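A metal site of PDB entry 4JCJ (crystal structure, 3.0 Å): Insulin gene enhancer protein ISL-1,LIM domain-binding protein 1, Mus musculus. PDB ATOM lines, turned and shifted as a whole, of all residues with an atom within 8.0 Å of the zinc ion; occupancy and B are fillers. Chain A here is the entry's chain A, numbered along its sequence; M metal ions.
N of Cys 9 lies within hydrogen-bond range of O of Asn 14 (2.9 Å). SG of Cys 9 sits close to N of Gly 11. O of Gln 15 lies within hydrogen-bond range of NE2 of His 31 (3.1 Å). The backbone carbonyl oxygen (O) of Cys 12 is in hydrogen-bond range of the side-chain amide nitrogen (ND2) of Asn 14 (3.3 Å).
ND1 of His 31 binds the zinc ion, 2.1 Å away. SG of Cys 9 binds the zinc ion (2.3 Å). The side-chain sulfur (SG) of Cys 12 binds the zinc ion, at 2.3 Å. SG of Cys 34 is bound to the zinc ion, at 2.3 Å. The zinc ion has four donor atoms within binding distance.
Within 4 Å of the zinc ion: Cys 9, Cys 12, His 31 and Cys 34. Along chain A the residues within 4 Å of the zinc ion span positions 9 to 34. The nearest printed residue that does not touch the zinc ion is Gly 11 (4.8 Å).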
ATOM      1  N   LEU A   8     -28.656   6.071 -23.728  1.00  0.00           N
ATOM      2  CA  LEU A   8     -28.232   5.996 -25.120  1.00  0.00           C
ATOM      3  C   LEU A   8     -28.579   7.287 -25.835  1.00  0.00           C
ATOM      4  O   LEU A   8     -29.744   7.676 -25.913  1.00  0.00           O
ATOM      5  CB  LEU A   8     -28.881   4.787 -25.819  1.00  0.00           C
ATOM      6  N   CYS A   9     -27.569   7.963 -26.362  1.00  0.00           N
ATOM      7  CA  CYS A   9     -27.786   9.243 -27.033  1.00  0.00           C
ATOM      8  C   CYS A   9     -28.681   9.104 -28.284  1.00  0.00           C
ATOM      9  O   CYS A   9     -28.347   8.407 -29.238  1.00  0.00           O
ATOM     10  CB  CYS A   9     -26.450   9.856 -27.432  1.00  0.00           C
ATOM     11  SG  CYS A   9     -26.606  11.071 -28.684  1.00  0.00           S
ATOM     12  N   VAL A  10     -29.818   9.787 -28.279  1.00  0.00           N
ATOM     13  CA  VAL A  10     -30.807   9.621 -29.341  1.00  0.00           C
ATOM     14  C   VAL A  10     -30.297  10.005 -30.755  1.00  0.00           C
ATOM     15  O   VAL A  10     -30.819   9.554 -31.779  1.00  0.00           O
ATOM     16  CB  VAL A  10     -32.131  10.387 -28.992  1.00  0.00           C
ATOM     17  CG1 VAL A  10     -32.987  10.623 -30.225  1.00  0.00           C
ATOM     18  CG2 VAL A  10     -32.928   9.592 -27.941  1.00  0.00           C
ATOM     19  N   GLY A  11     -29.269  10.844 -30.806  1.00  0.00           N
ATOM     20  CA  GLY A  11     -28.750  11.333 -32.063  1.00  0.00           C
ATOM     21  C   GLY A  11     -27.978  10.254 -32.786  1.00  0.00           C
ATOM     22  O   GLY A  11     -28.164  10.060 -33.997  1.00  0.00           O
ATOM     23  N   CYS A  12     -27.123   9.570 -32.023  1.00  0.00           N
ATOM     24  CA  CYS A  12     -26.139   8.635 -32.569  1.00  0.00           C
ATOM     25  C   CYS A  12     -26.230   7.222 -32.012  1.00  0.00           C
ATOM     26  O   CYS A  12     -25.511   6.358 -32.462  1.00  0.00           O
ATOM     27  CB  CYS A  12     -24.737   9.159 -32.291  1.00  0.00           C
ATOM     28  SG  CYS A  12     -24.257   9.127 -30.547  1.00  0.00           S
ATOM     29  N   GLY A  13     -27.059   7.012 -31.001  1.00  0.00           N
ATOM     30  CA  GLY A  13     -27.292   5.686 -30.433  1.00  0.00           C
ATOM     31  C   GLY A  13     -26.279   5.154 -29.416  1.00  0.00           C
ATOM     32  O   GLY A  13     -26.552   4.136 -28.790  1.00  0.00           O
ATOM     33  N   ASN A  14     -25.138   5.815 -29.252  1.00  0.00           N
ATOM     34  CA  ASN A  14     -24.083   5.321 -28.357  1.00  0.00           C
ATOM     35  C   ASN A  14     -24.262   5.800 -26.926  1.00  0.00           C
ATOM     36  O   ASN A  14     -25.007   6.751 -26.698  1.00  0.00           O
ATOM     37  CB  ASN A  14     -22.719   5.795 -28.862  1.00  0.00           C
ATOM     38  CG  ASN A  14     -22.480   5.416 -30.317  1.00  0.00           C
ATOM     39  OD1 ASN A  14     -22.259   4.237 -30.642  1.00  0.00           O
ATOM     40  ND2 ASN A  14     -22.491   6.411 -31.196  1.00  0.00           N
ATOM     41  N   GLN A  15     -23.598   5.151 -25.963  1.00  0.00           N
ATOM     42  CA  GLN A  15     -23.707   5.553 -24.539  1.00  0.00           C
ATOM     43  C   GLN A  15     -23.172   6.969 -24.336  1.00  0.00           C
ATOM     44  O   GLN A  15     -22.222   7.365 -24.988  1.00  0.00           O
ATOM     45  CB  GLN A  15     -22.930   4.616 -23.601  1.00  0.00           C
ATOM     46  N   ILE A  16     -23.813   7.727 -23.437  1.00  0.00           N
ATOM     47  CA  ILE A  16     -23.352   9.063 -23.083  1.00  0.00           C
ATOM     48  C   ILE A  16     -22.461   9.003 -21.863  1.00  0.00           C
ATOM     49  O   ILE A  16     -22.941   8.725 -20.773  1.00  0.00           O
ATOM     50  CB  ILE A  16     -24.534  10.026 -22.771  1.00  0.00           C
ATOM     51  CG1 ILE A  16     -25.522  10.076 -23.933  1.00  0.00           C
ATOM     52  CG2 ILE A  16     -23.999  11.430 -22.487  1.00  0.00           C
ATOM     53  CD1 ILE A  16     -26.597  11.165 -23.818  1.00  0.00           C
ATOM     54  N   ASP A  18     -20.432  11.693 -20.921  1.00  0.00           N
ATOM     55  CA  ASP A  18     -20.068  13.072 -20.571  1.00  0.00           C
ATOM     56  C   ASP A  18     -20.501  13.371 -19.134  1.00  0.00           C
ATOM     57  O   ASP A  18     -21.272  12.612 -18.555  1.00  0.00           O
ATOM     58  CB  ASP A  18     -20.729  14.076 -21.513  1.00  0.00           C
ATOM     59  CG  ASP A  18     -20.380  13.832 -22.990  1.00  0.00           C
ATOM     60  OD1 ASP A  18     -19.292  13.290 -23.280  1.00  0.00           O
ATOM     61  OD2 ASP A  18     -21.207  14.209 -23.862  1.00  0.00           O
ATOM     62  N   GLU A  29     -32.690  11.914 -24.243  1.00  0.00           N
ATOM     63  CA  GLU A  29     -31.353  12.210 -23.689  1.00  0.00           C
ATOM     64  C   GLU A  29     -30.358  12.342 -24.840  1.00  0.00           C
ATOM     65  O   GLU A  29     -30.412  11.556 -25.775  1.00  0.00           O
ATOM     66  CB  GLU A  29     -30.904  11.101 -22.731  1.00  0.00           C
ATOM     67  N   TRP A  30     -29.472  13.327 -24.745  1.00  0.00           N
ATOM     68  CA  TRP A  30     -28.545  13.631 -25.838  1.00  0.00           C
ATOM     69  C   TRP A  30     -27.125  13.871 -25.399  1.00  0.00           C
ATOM     70  O   TRP A  30     -26.896  14.508 -24.392  1.00  0.00           O
ATOM     71  CB  TRP A  30     -28.957  14.910 -26.532  1.00  0.00           C
ATOM     72  CG  TRP A  30     -30.246  14.839 -27.169  1.00  0.00           C
ATOM     73  CD1 TRP A  30     -31.437  15.089 -26.600  1.00  0.00           C
ATOM     74  CD2 TRP A  30     -30.493  14.525 -28.524  1.00  0.00           C
ATOM     75  NE1 TRP A  30     -32.441  14.939 -27.517  1.00  0.00           N
ATOM     76  CE2 TRP A  30     -31.883  14.576 -28.716  1.00  0.00           C
ATOM     77  CE3 TRP A  30     -29.676  14.180 -29.607  1.00  0.00           C
ATOM     78  CZ2 TRP A  30     -32.479  14.310 -29.948  1.00  0.00           C
ATOM     79  CZ3 TRP A  30     -30.266  13.914 -30.817  1.00  0.00           C
ATOM     80  CH2 TRP A  30     -31.654  13.974 -30.987  1.00  0.00           C
ATOM     81  N   HIS A  31     -26.179  13.400 -26.184  1.00  0.00           N
ATOM     82  CA  HIS A  31     -24.852  13.975 -26.192  1.00  0.00           C
ATOM     83  C   HIS A  31     -25.048  15.436 -26.495  1.00  0.00           C
ATOM     84  O   HIS A  31     -25.916  15.792 -27.285  1.00  0.00           O
ATOM     85  CB  HIS A  31     -23.997  13.362 -27.304  1.00  0.00           C
ATOM     86  CG  HIS A  31     -23.444  12.013 -26.977  1.00  0.00           C
ATOM     87  ND1 HIS A  31     -23.373  10.993 -27.892  1.00  0.00           N
ATOM     88  CD2 HIS A  31     -22.944  11.517 -25.828  1.00  0.00           C
ATOM     89  CE1 HIS A  31     -22.853   9.931 -27.327  1.00  0.00           C
ATOM     90  NE2 HIS A  31     -22.574  10.218 -26.066  1.00  0.00           N
ATOM     91  N   ALA A  32     -24.240  16.287 -25.891  1.00  0.00           N
ATOM     92  CA  ALA A  32     -24.404  17.720 -26.125  1.00  0.00           C
ATOM     93  C   ALA A  32     -24.086  18.092 -27.553  1.00  0.00           C
ATOM     94  O   ALA A  32     -24.686  19.022 -28.093  1.00  0.00           O
ATOM     95  CB  ALA A  32     -23.559  18.528 -25.177  1.00  0.00           C
ATOM     96  N   ALA A  33     -23.158  17.349 -28.149  1.00  0.00           N
ATOM     97  CA  ALA A  33     -22.733  17.565 -29.535  1.00  0.00           C
ATOM     98  C   ALA A  33     -23.707  17.033 -30.576  1.00  0.00           C
ATOM     99  O   ALA A  33     -23.624  17.411 -31.743  1.00  0.00           O
ATOM    100  CB  ALA A  33     -21.385  16.918 -29.775  1.00  0.00           C
ATOM    101  N   CYS A  34     -24.620  16.155 -30.182  1.00  0.00           N
ATOM    102  CA  CYS A  34     -25.527  15.565 -31.145  1.00  0.00           C
ATOM    103  C   CYS A  34     -26.876  16.262 -31.172  1.00  0.00           C
ATOM    104  O   CYS A  34     -27.750  15.887 -31.955  1.00  0.00           O
ATOM    105  CB  CYS A  34     -25.703  14.075 -30.870  1.00  0.00           C
ATOM    106  SG  CYS A  34     -24.204  13.062 -31.094  1.00  0.00           S
ATOM    107  N   LEU A  35     -27.061  17.270 -30.323  1.00  0.00           N
ATOM    108  CA  LEU A  35     -28.315  18.006 -30.301  1.00  0.00           C
ATOM    109  C   LEU A  35     -28.247  19.229 -31.248  1.00  0.00           C
ATOM    110  O   LEU A  35     -28.031  20.357 -30.821  1.00  0.00           O
ATOM    111  CB  LEU A  35     -28.659  18.404 -28.864  1.00  0.00           C
ATOM    112  CG  LEU A  35     -30.121  18.842 -28.638  1.00  0.00           C
ATOM    113  CD1 LEU A  35     -31.034  17.673 -28.795  1.00  0.00           C
ATOM    114  CD2 LEU A  35     -30.304  19.405 -27.263  1.00  0.00           C
HETATM  115 ZN    ZN M   1     -24.521  11.257 -29.667  1.00  0.00          ZN
